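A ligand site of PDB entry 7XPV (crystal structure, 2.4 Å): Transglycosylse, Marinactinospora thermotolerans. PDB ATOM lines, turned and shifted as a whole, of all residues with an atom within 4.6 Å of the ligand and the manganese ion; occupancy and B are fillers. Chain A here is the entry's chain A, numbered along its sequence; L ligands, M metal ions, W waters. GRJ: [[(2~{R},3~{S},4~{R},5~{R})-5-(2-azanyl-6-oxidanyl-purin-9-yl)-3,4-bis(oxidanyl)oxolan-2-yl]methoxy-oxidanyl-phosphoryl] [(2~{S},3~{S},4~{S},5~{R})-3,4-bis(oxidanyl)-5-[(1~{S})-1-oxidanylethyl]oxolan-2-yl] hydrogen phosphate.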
ATOM      1  N   THR A  32     -21.450 -20.432  17.475  1.00  0.00           N
ATOM      2  CA  THR A  32     -21.975 -19.412  18.384  1.00  0.00           C
ATOM      3  C   THR A  32     -21.112 -18.158  18.281  1.00  0.00           C
ATOM      4  O   THR A  32     -19.880 -18.252  18.189  1.00  0.00           O
ATOM      5  CB  THR A  32     -22.032 -19.926  19.824  1.00  0.00           C
ATOM      6  OG1 THR A  32     -22.564 -18.900  20.676  1.00  0.00           O
ATOM      7  CG2 THR A  32     -20.652 -20.327  20.328  1.00  0.00           C
ATOM      8  N   THR A  33     -21.753 -16.994  18.288  1.00  0.00           N
ATOM      9  CA  THR A  33     -21.035 -15.757  18.031  1.00  0.00           C
ATOM     10  C   THR A  33     -21.781 -14.586  18.641  1.00  0.00           C
ATOM     11  O   THR A  33     -22.991 -14.640  18.885  1.00  0.00           O
ATOM     12  CB  THR A  33     -20.844 -15.518  16.525  1.00  0.00           C
ATOM     13  OG1 THR A  33     -20.191 -14.260  16.304  1.00  0.00           O
ATOM     14  CG2 THR A  33     -22.187 -15.511  15.809  1.00  0.00           C
ATOM     15  N   ILE A  34     -21.025 -13.507  18.891  1.00  0.00           N
ATOM     16  CA  ILE A  34     -21.555 -12.224  19.320  1.00  0.00           C
ATOM     17  C   ILE A  34     -21.222 -11.114  18.339  1.00  0.00           C
ATOM     18  O   ILE A  34     -21.392  -9.934  18.652  1.00  0.00           O
ATOM     19  CB  ILE A  34     -21.070 -11.868  20.734  1.00  0.00           C
ATOM     20  CG1 ILE A  34     -19.544 -11.829  20.778  1.00  0.00           C
ATOM     21  CG2 ILE A  34     -21.625 -12.849  21.761  1.00  0.00           C
ATOM     22  CD1 ILE A  34     -18.980 -11.371  22.114  1.00  0.00           C
ATOM     23  N   ILE A  57     -25.801 -19.579  16.935  1.00  0.00           N
ATOM     24  CA  ILE A  57     -26.342 -19.452  18.289  1.00  0.00           C
ATOM     25  C   ILE A  57     -25.974 -18.079  18.842  1.00  0.00           C
ATOM     26  O   ILE A  57     -24.844 -17.878  19.302  1.00  0.00           O
ATOM     27  CB  ILE A  57     -25.819 -20.571  19.208  1.00  0.00           C
ATOM     28  CG1 ILE A  57     -26.169 -21.949  18.631  1.00  0.00           C
ATOM     29  CG2 ILE A  57     -26.401 -20.427  20.603  1.00  0.00           C
ATOM     30  CD1 ILE A  57     -27.646 -22.209  18.523  1.00  0.00           C
ATOM     31  N   ASP A  59     -26.405 -14.741  21.568  1.00  0.00           N
ATOM     32  CA  ASP A  59     -26.466 -14.604  23.021  1.00  0.00           C
ATOM     33  C   ASP A  59     -27.217 -13.317  23.361  1.00  0.00           C
ATOM     34  O   ASP A  59     -27.734 -12.622  22.479  1.00  0.00           O
ATOM     35  CB  ASP A  59     -25.060 -14.610  23.618  1.00  0.00           C
ATOM     36  CG  ASP A  59     -25.025 -15.119  25.049  1.00  0.00           C
ATOM     37  OD1 ASP A  59     -26.024 -14.904  25.780  1.00  0.00           O
ATOM     38  OD2 ASP A  59     -24.014 -15.732  25.444  1.00  0.00           O
ATOM     39  N   ASN A  61     -25.876 -10.591  24.666  1.00  0.00           N
ATOM     40  CA  ASN A  61     -25.042  -9.456  24.278  1.00  0.00           C
ATOM     41  C   ASN A  61     -24.682  -9.475  22.804  1.00  0.00           C
ATOM     42  O   ASN A  61     -23.661  -8.880  22.411  1.00  0.00           O
ATOM     43  CB  ASN A  61     -23.769  -9.428  25.136  1.00  0.00           C
ATOM     44  CG  ASN A  61     -22.927 -10.684  24.983  1.00  0.00           C
ATOM     45  OD1 ASN A  61     -23.462 -11.771  24.785  1.00  0.00           O
ATOM     46  ND2 ASN A  61     -21.617 -10.535  25.083  1.00  0.00           N
ATOM     47  N   HIS A 104     -23.957 -14.972  28.119  1.00  0.00           N
ATOM     48  CA  HIS A 104     -22.707 -14.219  28.024  1.00  0.00           C
ATOM     49  C   HIS A 104     -21.498 -15.148  28.003  1.00  0.00           C
ATOM     50  O   HIS A 104     -20.469 -14.886  28.628  1.00  0.00           O
ATOM     51  CB  HIS A 104     -22.589 -13.188  29.153  1.00  0.00           C
ATOM     52  CG  HIS A 104     -23.682 -12.173  29.163  1.00  0.00           C
ATOM     53  ND1 HIS A 104     -25.001 -12.484  29.409  1.00  0.00           N
ATOM     54  CD2 HIS A 104     -23.654 -10.828  28.966  1.00  0.00           C
ATOM     55  CE1 HIS A 104     -25.736 -11.393  29.364  1.00  0.00           C
ATOM     56  NE2 HIS A 104     -24.946 -10.368  29.095  1.00  0.00           N
ATOM     57  N   SER A 105     -21.625 -16.258  27.278  1.00  0.00           N
ATOM     58  CA  SER A 105     -20.584 -17.279  27.231  1.00  0.00           C
ATOM     59  C   SER A 105     -20.691 -18.061  25.939  1.00  0.00           C
ATOM     60  O   SER A 105     -21.793 -18.264  25.411  1.00  0.00           O
ATOM     61  CB  SER A 105     -20.682 -18.229  28.436  1.00  0.00           C
ATOM     62  OG  SER A 105     -19.838 -19.351  28.266  1.00  0.00           O
ATOM     63  N   ASP A 106     -19.542 -18.507  25.423  1.00  0.00           N
ATOM     64  CA  ASP A 106     -19.528 -19.370  24.252  1.00  0.00           C
ATOM     65  C   ASP A 106     -20.002 -20.784  24.553  1.00  0.00           C
ATOM     66  O   ASP A 106     -20.040 -21.616  23.640  1.00  0.00           O
ATOM     67  CB  ASP A 106     -18.124 -19.412  23.643  1.00  0.00           C
ATOM     68  CG  ASP A 106     -17.119 -20.126  24.523  1.00  0.00           C
ATOM     69  OD1 ASP A 106     -17.269 -20.062  25.763  1.00  0.00           O
ATOM     70  OD2 ASP A 106     -16.195 -20.759  23.972  1.00  0.00           O
ATOM     71  N   ARG A 108     -22.911 -21.529  24.912  1.00  0.00           N
ATOM     72  CA  ARG A 108     -24.198 -21.667  24.245  1.00  0.00           C
ATOM     73  C   ARG A 108     -24.131 -22.464  22.959  1.00  0.00           C
ATOM     74  O   ARG A 108     -25.180 -22.759  22.378  1.00  0.00           O
ATOM     75  CB  ARG A 108     -24.786 -20.286  23.964  1.00  0.00           C
ATOM     76  CG  ARG A 108     -24.951 -19.415  25.198  1.00  0.00           C
ATOM     77  CD  ARG A 108     -26.208 -18.563  25.112  1.00  0.00           C
ATOM     78  NE  ARG A 108     -27.420 -19.371  25.083  1.00  0.00           N
ATOM     79  CZ  ARG A 108     -28.041 -19.817  26.167  1.00  0.00           C
ATOM     80  NH1 ARG A 108     -27.590 -19.572  27.379  1.00  0.00           N
ATOM     81  NH2 ARG A 108     -29.150 -20.541  26.018  1.00  0.00           N
ATOM     82  N   ARG A 109     -22.929 -22.837  22.504  1.00  0.00           N
ATOM     83  CA  ARG A 109     -22.814 -23.719  21.349  1.00  0.00           C
ATOM     84  C   ARG A 109     -23.431 -25.085  21.622  1.00  0.00           C
ATOM     85  O   ARG A 109     -23.736 -25.822  20.667  1.00  0.00           O
ATOM     86  CB  ARG A 109     -21.349 -23.871  20.937  1.00  0.00           C
ATOM     87  CG  ARG A 109     -20.503 -24.621  21.935  1.00  0.00           C
ATOM     88  CD  ARG A 109     -19.046 -24.641  21.498  1.00  0.00           C
ATOM     89  NE  ARG A 109     -18.411 -23.337  21.633  1.00  0.00           N
ATOM     90  CZ  ARG A 109     -17.263 -23.006  21.053  1.00  0.00           C
ATOM     91  NH1 ARG A 109     -16.622 -23.847  20.252  1.00  0.00           N
ATOM     92  NH2 ARG A 109     -16.742 -21.796  21.276  1.00  0.00           N
ATOM     93  N   ASP A 128     -16.013 -21.895  14.873  1.00  0.00           N
ATOM     94  CA  ASP A 128     -16.094 -20.556  15.444  1.00  0.00           C
ATOM     95  C   ASP A 128     -16.299 -19.543  14.328  1.00  0.00           C
ATOM     96  O   ASP A 128     -16.229 -19.871  13.140  1.00  0.00           O
ATOM     97  CB  ASP A 128     -14.836 -20.228  16.247  1.00  0.00           C
ATOM     98  CG  ASP A 128     -14.724 -21.039  17.526  1.00  0.00           C
ATOM     99  OD1 ASP A 128     -15.771 -21.405  18.087  1.00  0.00           O
ATOM    100  OD2 ASP A 128     -13.580 -21.300  17.963  1.00  0.00           O
ATOM    101  N   ASP A 129     -16.583 -18.298  14.719  1.00  0.00           N
ATOM    102  CA  ASP A 129     -16.854 -17.243  13.747  1.00  0.00           C
ATOM    103  C   ASP A 129     -15.580 -16.657  13.127  1.00  0.00           C
ATOM    104  O   ASP A 129     -15.663 -15.596  12.495  1.00  0.00           O
ATOM    105  CB  ASP A 129     -17.683 -16.126  14.397  1.00  0.00           C
ATOM    106  CG  ASP A 129     -16.961 -15.461  15.563  1.00  0.00           C
ATOM    107  OD1 ASP A 129     -15.832 -15.856  15.894  1.00  0.00           O
ATOM    108  OD2 ASP A 129     -17.557 -14.540  16.165  1.00  0.00           O
ATOM    109  N   ASP A 130     -14.440 -17.309  13.296  1.00  0.00           N
ATOM    110  CA  ASP A 130     -13.192 -16.844  12.697  1.00  0.00           C
ATOM    111  C   ASP A 130     -12.434 -17.949  11.979  1.00  0.00           C
ATOM    112  O   ASP A 130     -11.294 -17.739  11.572  1.00  0.00           O
ATOM    113  CB  ASP A 130     -12.290 -16.196  13.759  1.00  0.00           C
ATOM    114  CG  ASP A 130     -11.968 -17.130  14.892  1.00  0.00           C
ATOM    115  OD1 ASP A 130     -12.722 -18.103  15.101  1.00  0.00           O
ATOM    116  OD2 ASP A 130     -10.960 -16.898  15.597  1.00  0.00           O
ATOM    117  N   ASN A 131     -13.032 -19.125  11.818  1.00  0.00           N
ATOM    118  CA  ASN A 131     -12.449 -20.217  11.056  1.00  0.00           C
ATOM    119  C   ASN A 131     -13.138 -20.291   9.704  1.00  0.00           C
ATOM    120  O   ASN A 131     -14.354 -20.457   9.628  1.00  0.00           O
ATOM    121  CB  ASN A 131     -12.584 -21.545  11.815  1.00  0.00           C
ATOM    122  CG  ASN A 131     -11.796 -21.568  13.111  1.00  0.00           C
ATOM    123  OD1 ASN A 131     -10.648 -22.014  13.150  1.00  0.00           O
ATOM    124  ND2 ASN A 131     -12.406 -21.067  14.189  1.00  0.00           N
ATOM    125  N   ARG A 178      -3.193 -26.660  21.941  1.00  0.00           N
ATOM    126  CA  ARG A 178      -3.809 -26.296  23.210  1.00  0.00           C
ATOM    127  C   ARG A 178      -4.480 -27.507  23.838  1.00  0.00           C
ATOM    128  O   ARG A 178      -5.204 -28.253  23.169  1.00  0.00           O
ATOM    129  CB  ARG A 178      -4.825 -25.169  22.999  1.00  0.00           C
ATOM    130  CG  ARG A 178      -5.535 -24.709  24.266  1.00  0.00           C
ATOM    131  CD  ARG A 178      -6.467 -23.551  23.958  1.00  0.00           C
ATOM    132  NE  ARG A 178      -7.369 -23.864  22.857  1.00  0.00           N
ATOM    133  CZ  ARG A 178      -8.611 -24.309  23.002  1.00  0.00           C
ATOM    134  NH1 ARG A 178      -9.139 -24.480  24.206  1.00  0.00           N
ATOM    135  NH2 ARG A 178      -9.330 -24.586  21.927  1.00  0.00           N
ATOM    136  N   ASP A 214      -4.176 -23.394  16.792  1.00  0.00           N
ATOM    137  CA  ASP A 214      -4.802 -23.565  18.101  1.00  0.00           C
ATOM    138  C   ASP A 214      -3.774 -24.004  19.137  1.00  0.00           C
ATOM    139  O   ASP A 214      -3.609 -25.205  19.381  1.00  0.00           O
ATOM    140  CB  ASP A 214      -5.943 -24.577  18.032  1.00  0.00           C
ATOM    141  CG  ASP A 214      -6.687 -24.711  19.346  1.00  0.00           C
ATOM    142  OD1 ASP A 214      -6.611 -23.774  20.174  1.00  0.00           O
ATOM    143  OD2 ASP A 214      -7.337 -25.753  19.570  1.00  0.00           O
ATOM    144  N   GLN A 248     -13.343 -25.724  17.111  1.00  0.00           N
ATOM    145  CA  GLN A 248     -13.336 -24.677  16.094  1.00  0.00           C
ATOM    146  C   GLN A 248     -13.294 -25.219  14.669  1.00  0.00           C
ATOM    147  O   GLN A 248     -13.590 -24.471  13.736  1.00  0.00           O
ATOM    148  CB  GLN A 248     -12.137 -23.736  16.310  1.00  0.00           C
ATOM    149  CG  GLN A 248     -10.788 -24.427  16.238  1.00  0.00           C
ATOM    150  CD  GLN A 248      -9.655 -23.507  16.663  1.00  0.00           C
ATOM    151  OE1 GLN A 248      -9.385 -23.347  17.851  1.00  0.00           O
ATOM    152  NE2 GLN A 248      -8.999 -22.903  15.684  1.00  0.00           N
ATOM    153  N   PHE A 262     -19.853 -29.373  25.595  1.00  0.00           N
ATOM    154  CA  PHE A 262     -18.899 -28.306  25.880  1.00  0.00           C
ATOM    155  C   PHE A 262     -18.976 -27.935  27.357  1.00  0.00           C
ATOM    156  O   PHE A 262     -19.988 -27.379  27.810  1.00  0.00           O
ATOM    157  CB  PHE A 262     -19.203 -27.104  24.990  1.00  0.00           C
ATOM    158  CG  PHE A 262     -18.148 -26.025  25.006  1.00  0.00           C
ATOM    159  CD1 PHE A 262     -17.062 -26.094  24.142  1.00  0.00           C
ATOM    160  CD2 PHE A 262     -18.261 -24.935  25.849  1.00  0.00           C
ATOM    161  CE1 PHE A 262     -16.100 -25.098  24.146  1.00  0.00           C
ATOM    162  CE2 PHE A 262     -17.305 -23.934  25.847  1.00  0.00           C
ATOM    163  CZ  PHE A 262     -16.225 -24.015  24.995  1.00  0.00           C
ATOM    164  N   GLU A 275     -11.128 -20.723  32.423  1.00  0.00           N
ATOM    165  CA  GLU A 275     -11.813 -20.414  31.176  1.00  0.00           C
ATOM    166  C   GLU A 275     -10.980 -20.969  30.034  1.00  0.00           C
ATOM    167  O   GLU A 275      -9.884 -21.492  30.230  1.00  0.00           O
ATOM    168  CB  GLU A 275     -12.050 -18.912  31.026  1.00  0.00           C
ATOM    169  CG  GLU A 275     -13.462 -18.449  31.356  1.00  0.00           C
ATOM    170  CD  GLU A 275     -14.486 -18.909  30.337  1.00  0.00           C
ATOM    171  OE1 GLU A 275     -14.094 -19.365  29.239  1.00  0.00           O
ATOM    172  OE2 GLU A 275     -15.699 -18.816  30.633  1.00  0.00           O
ATOM    173  N   ARG A 276     -11.535 -20.870  28.818  1.00  0.00           N
ATOM    174  CA  ARG A 276     -10.880 -21.213  27.560  1.00  0.00           C
ATOM    175  C   ARG A 276     -10.571 -22.699  27.406  1.00  0.00           C
ATOM    176  O   ARG A 276      -9.899 -23.085  26.436  1.00  0.00           O
ATOM    177  CB  ARG A 276      -9.582 -20.404  27.361  1.00  0.00           C
ATOM    178  CG  ARG A 276      -9.807 -18.897  27.256  1.00  0.00           C
ATOM    179  CD  ARG A 276      -8.511 -18.173  26.911  1.00  0.00           C
ATOM    180  NE  ARG A 276      -7.791 -18.842  25.838  1.00  0.00           N
ATOM    181  CZ  ARG A 276      -8.072 -18.707  24.551  1.00  0.00           C
ATOM    182  NH1 ARG A 276      -9.044 -17.907  24.131  1.00  0.00           N
ATOM    183  NH2 ARG A 276      -7.361 -19.387  23.651  1.00  0.00           N
ATOM    184  N   GLY A 278     -13.177 -25.184  27.728  1.00  0.00           N
ATOM    185  CA  GLY A 278     -14.429 -25.922  27.616  1.00  0.00           C
ATOM    186  C   GLY A 278     -14.363 -27.019  26.574  1.00  0.00           C
ATOM    187  O   GLY A 278     -14.906 -28.112  26.776  1.00  0.00           O
ATOM    188  N   ASP A 279     -13.702 -26.757  25.449  1.00  0.00           N
ATOM    189  CA  ASP A 279     -13.555 -27.760  24.408  1.00  0.00           C
ATOM    190  C   ASP A 279     -12.368 -28.673  24.633  1.00  0.00           C
ATOM    191  O   ASP A 279     -12.290 -29.725  23.982  1.00  0.00           O
ATOM    192  CB  ASP A 279     -13.439 -27.082  23.037  1.00  0.00           C
ATOM    193  CG  ASP A 279     -12.323 -26.062  22.985  1.00  0.00           C
ATOM    194  OD1 ASP A 279     -11.963 -25.518  24.049  1.00  0.00           O
ATOM    195  OD2 ASP A 279     -11.806 -25.798  21.878  1.00  0.00           O
ATOM    196  N   HIS A 306      -7.506 -19.424   9.964  1.00  0.00           N
ATOM    197  CA  HIS A 306      -7.810 -18.964  11.316  1.00  0.00           C
ATOM    198  C   HIS A 306      -7.251 -17.556  11.523  1.00  0.00           C
ATOM    199  O   HIS A 306      -6.221 -17.377  12.192  1.00  0.00           O
ATOM    200  CB  HIS A 306      -7.267 -19.933  12.368  1.00  0.00           C
ATOM    201  CG  HIS A 306      -7.683 -19.594  13.765  1.00  0.00           C
ATOM    202  ND1 HIS A 306      -6.964 -19.999  14.870  1.00  0.00           N
ATOM    203  CD2 HIS A 306      -8.735 -18.887  14.243  1.00  0.00           C
ATOM    204  CE1 HIS A 306      -7.552 -19.564  15.967  1.00  0.00           C
ATOM    205  NE2 HIS A 306      -8.631 -18.880  15.607  1.00  0.00           N
ATOM    206  N   ARG A 308      -7.437 -15.232  13.801  1.00  0.00           N
ATOM    207  CA  ARG A 308      -7.988 -15.221  15.161  1.00  0.00           C
ATOM    208  C   ARG A 308      -8.444 -13.822  15.567  1.00  0.00           C
ATOM    209  O   ARG A 308      -7.838 -12.824  15.193  1.00  0.00           O
ATOM    210  CB  ARG A 308      -6.943 -15.732  16.150  1.00  0.00           C
ATOM    211  CG  ARG A 308      -7.507 -16.042  17.523  1.00  0.00           C
ATOM    212  CD  ARG A 308      -6.443 -15.982  18.599  1.00  0.00           C
ATOM    213  NE  ARG A 308      -6.989 -16.301  19.911  1.00  0.00           N
ATOM    214  CZ  ARG A 308      -6.345 -16.113  21.053  1.00  0.00           C
ATOM    215  NH1 ARG A 308      -5.130 -15.585  21.083  1.00  0.00           N
ATOM    216  NH2 ARG A 308      -6.931 -16.461  22.190  1.00  0.00           N
ATOM    217  N   ASN A 309      -9.535 -13.774  16.330  1.00  0.00           N
ATOM    218  CA  ASN A 309     -10.016 -12.511  16.862  1.00  0.00           C
ATOM    219  C   ASN A 309      -8.963 -11.886  17.776  1.00  0.00           C
ATOM    220  O   ASN A 309      -8.130 -12.580  18.373  1.00  0.00           O
ATOM    221  CB  ASN A 309     -11.320 -12.730  17.643  1.00  0.00           C
ATOM    222  CG  ASN A 309     -12.428 -13.308  16.779  1.00  0.00           C
ATOM    223  OD1 ASN A 309     -12.534 -12.992  15.592  1.00  0.00           O
ATOM    224  ND2 ASN A 309     -13.256 -14.157  17.371  1.00  0.00           N
ATOM    225  N   HIS A 311      -7.181 -10.665  20.824  1.00  0.00           N
ATOM    226  CA  HIS A 311      -7.233 -11.097  22.211  1.00  0.00           C
ATOM    227  C   HIS A 311      -6.125 -10.433  23.017  1.00  0.00           C
ATOM    228  O   HIS A 311      -5.066 -10.081  22.481  1.00  0.00           O
ATOM    229  CB  HIS A 311      -7.110 -12.618  22.345  1.00  0.00           C
ATOM    230  CG  HIS A 311      -8.405 -13.353  22.125  1.00  0.00           C
ATOM    231  ND1 HIS A 311      -8.964 -13.534  20.881  1.00  0.00           N
ATOM    232  CD2 HIS A 311      -9.242 -13.952  23.008  1.00  0.00           C
ATOM    233  CE1 HIS A 311     -10.091 -14.214  20.999  1.00  0.00           C
ATOM    234  NE2 HIS A 311     -10.283 -14.482  22.271  1.00  0.00           N
HETATM  235  N1  GRJ L   1     -17.762 -14.549  23.549  1.00  0.00           N
HETATM  236  N3  GRJ L   1     -21.369 -15.392  24.046  1.00  0.00           N
HETATM  237  C4  GRJ L   1     -11.064 -21.782  22.207  1.00  0.00           C
HETATM  238  C5  GRJ L   1     -11.860 -20.820  21.349  1.00  0.00           C
HETATM  239  C6  GRJ L   1     -14.415 -18.366  20.268  1.00  0.00           C
HETATM  240  C7  GRJ L   1     -15.891 -18.230  19.917  1.00  0.00           C
HETATM  241  C8  GRJ L   1     -16.102 -17.127  18.890  1.00  0.00           C
HETATM  242  C10 GRJ L   1     -17.610 -16.863  20.712  1.00  0.00           C
HETATM  243  C13 GRJ L   1     -19.151 -15.955  22.451  1.00  0.00           C
HETATM  244  C15 GRJ L   1     -20.249 -14.730  24.369  1.00  0.00           C
HETATM  245  N   GRJ L   1     -17.948 -16.010  21.873  1.00  0.00           N
HETATM  246  C   GRJ L   1     -13.788 -18.772  24.944  1.00  0.00           C
HETATM  247  O   GRJ L   1     -12.399 -19.852  22.260  1.00  0.00           O
HETATM  248  C1  GRJ L   1     -12.509 -19.566  24.679  1.00  0.00           C
HETATM  249  C11 GRJ L   1     -17.125 -15.178  22.532  1.00  0.00           C
HETATM  250  C12 GRJ L   1     -19.034 -14.990  23.556  1.00  0.00           C
HETATM  251  C14 GRJ L   1     -21.423 -16.259  23.016  1.00  0.00           C
HETATM  252  C2  GRJ L   1     -12.668 -20.510  23.500  1.00  0.00           C
HETATM  253  C3  GRJ L   1     -11.702 -21.685  23.584  1.00  0.00           C
HETATM  254  C9  GRJ L   1     -16.932 -16.073  19.604  1.00  0.00           C
HETATM  255  N2  GRJ L   1     -20.351 -16.543  22.229  1.00  0.00           N
HETATM  256  N4  GRJ L   1     -22.597 -16.891  22.760  1.00  0.00           N
HETATM  257  O1  GRJ L   1     -11.076 -20.233  20.303  1.00  0.00           O
HETATM  258  O10 GRJ L   1     -17.882 -15.499  18.709  1.00  0.00           O
HETATM  259  O11 GRJ L   1     -16.835 -17.639  17.771  1.00  0.00           O
HETATM  260  O12 GRJ L   1      -9.696 -21.386  22.280  1.00  0.00           O
HETATM  261  O13 GRJ L   1     -12.428 -22.880  23.889  1.00  0.00           O
HETATM  262  O14 GRJ L   1     -11.427 -18.655  24.424  1.00  0.00           O
HETATM  263  O2  GRJ L   1      -9.448 -18.596  19.249  1.00  0.00           O
HETATM  264  O3  GRJ L   1      -9.257 -18.984  21.729  1.00  0.00           O
HETATM  265  O4  GRJ L   1     -11.284 -17.646  20.685  1.00  0.00           O
HETATM  266  O5  GRJ L   1     -11.819 -15.757  19.101  1.00  0.00           O
HETATM  267  O6  GRJ L   1     -12.043 -18.092  18.203  1.00  0.00           O
HETATM  268  O7  GRJ L   1     -13.748 -17.146  19.964  1.00  0.00           O
HETATM  269  O8  GRJ L   1     -16.659 -17.865  21.074  1.00  0.00           O
HETATM  270  O9  GRJ L   1     -20.226 -13.933  25.317  1.00  0.00           O
HETATM  271  P   GRJ L   1     -10.247 -18.864  20.464  1.00  0.00           P
HETATM  272  P1  GRJ L   1     -12.214 -17.130  19.476  1.00  0.00           P
HETATM  273 MN    MN M   1     -10.670 -18.353  16.977  1.00  0.00          MN
HETATM  274  O   HOH W   1     -16.642 -11.770  25.121  1.00  0.00           O
HETATM  275  O   HOH W   2     -12.516 -16.712  22.861  1.00  0.00           O
HETATM  276  O   HOH W   3     -11.166 -23.586  19.471  1.00  0.00           O
HETATM  277  O   HOH W   4     -13.873 -22.364  27.014  1.00  0.00           O
HETATM  278  O   HOH W   5      -6.901 -20.736  19.849  1.00  0.00           O
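Residues that only touch the ligand: Thr 33, Ile 34, Asn 61, Asp 106, Arg 109, Asp 128 and His 311. 19 residues have an atom within 4 Å of the ligand: Thr 32, Thr 33, Ile 34, Asp 59, Asn 61, His 104, Ser 105, Asp 106, Arg 109, Asp 128, Asp 129, Asp 130, Arg 178, Arg 276, Asp 279, His 306, Arg 308, Asn 309 and His 311. The nearest printed residue that does not touch the ligand is Phe 262 (4.1 Å).
The guanidinium group of Arg 276 is in salt-bridge range of an oxygen (O3) of the ligand (2.6 Å). An oxygen (O12) of the ligand sits close to the guanidinium group of Arg 178 (3.2 Å). The side-chain carboxylate (OD1) of Asp 279 lies within hydrogen-bond range of an oxygen (O13) of the ligand. ND2 of Asn 309 sits at hydrogen-bond distance from O5 of the ligand (2.8 Å). An oxygen (O9) of the ligand sits close to the backbone carbonyl oxygen (O) of His 104, 3.5 Å away. An oxygen (O9) of the ligand sits at hydrogen-bond distance from the backbone NH (N) of Ser 105 (3.3 Å). OD2 of Asp 59 is in hydrogen-bond range of N4 of the ligand, at 3.2 Å. The side-chain hydroxyl of Thr 32 sits at hydrogen-bond distance from a nitrogen (N4) of the ligand, 2.9 Å away. An oxygen (O11) of the ligand is in hydrogen-bond range of the backbone carbonyl oxygen of Thr 32, 3.1 Å away. OD2 of Asp 129 sits at hydrogen-bond distance from O10 of the ligand. An oxygen (O11) of the ligand lies close to the backbone NH (N) of Asp 129, 3.1 Å away. O3 of the ligand lies within salt-bridge range of NH2 of Arg 308, at 3.5 Å. O of Ser 105 sits at hydrogen-bond distance from N4 of the ligand.
The manganese ion is bound by an oxygen (O6) of the ligand (1.9 Å). OD2 of Asp 130 binds the manganese ion (2.0 Å). The manganese ion is bound by NE2 of His 306 (2.5 Å). An oxygen (O2) of the ligand binds the manganese ion (2.6 Å). Slightly farther from the manganese ion lies the side-chain carboxylate (OD1) of Asp 130 (2.8 Å).
Merely in contact with the manganese ion: Arg 308 (3.96 Å). Three residues have an atom within 4 Å of the manganese ion: Asp 130, His 306 and Arg 308.
Water W2 lies within hydrogen-bond range of an oxygen (O4) of the ligand (2.7 Å) and a ring nitrogen (NE2) of His 311 (3.2 Å). Water W5 lies within hydrogen-bond range of OD1 of Asp 214 (3.1 Å) and O3 of the ligand (3.5 Å). Water W4 lies within hydrogen-bond range of N of Gly 278 (3.0 Å), N of Arg 276 (3.3 Å) and O13 of the ligand (3.5 Å).
OG1 of Thr 32 sits at hydrogen-bond distance from O of Ile 57, 2.9 Å away. OD1 of Asp 129 lies within hydrogen-bond range of ND2 of Asn 309 (3.4 Å). The side-chain carboxylate (OD2) of Asp 59 lies within hydrogen-bond range of the backbone NH (N) of Ser 105. The guanidinium group (NH1) of Arg 178 is in hydrogen-bond range of the backbone carbonyl oxygen (O) of Arg 276 (2.7 Å). N of Thr 33 lies within hydrogen-bond range of O of Ile 57, 3.4 Å away. The side-chain carboxylate (OD2) of Asp 279 lies within salt-bridge range of the guanidinium group (NH2) of Arg 178 (2.8 Å). NE of Arg 178 lies within salt-bridge range of OD1 of Asp 214 (2.8 Å). The side-chain carboxylate of Asp 129 sits at hydrogen-bond distance from the side-chain hydroxyl of Thr 33, at 2.7 Å.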
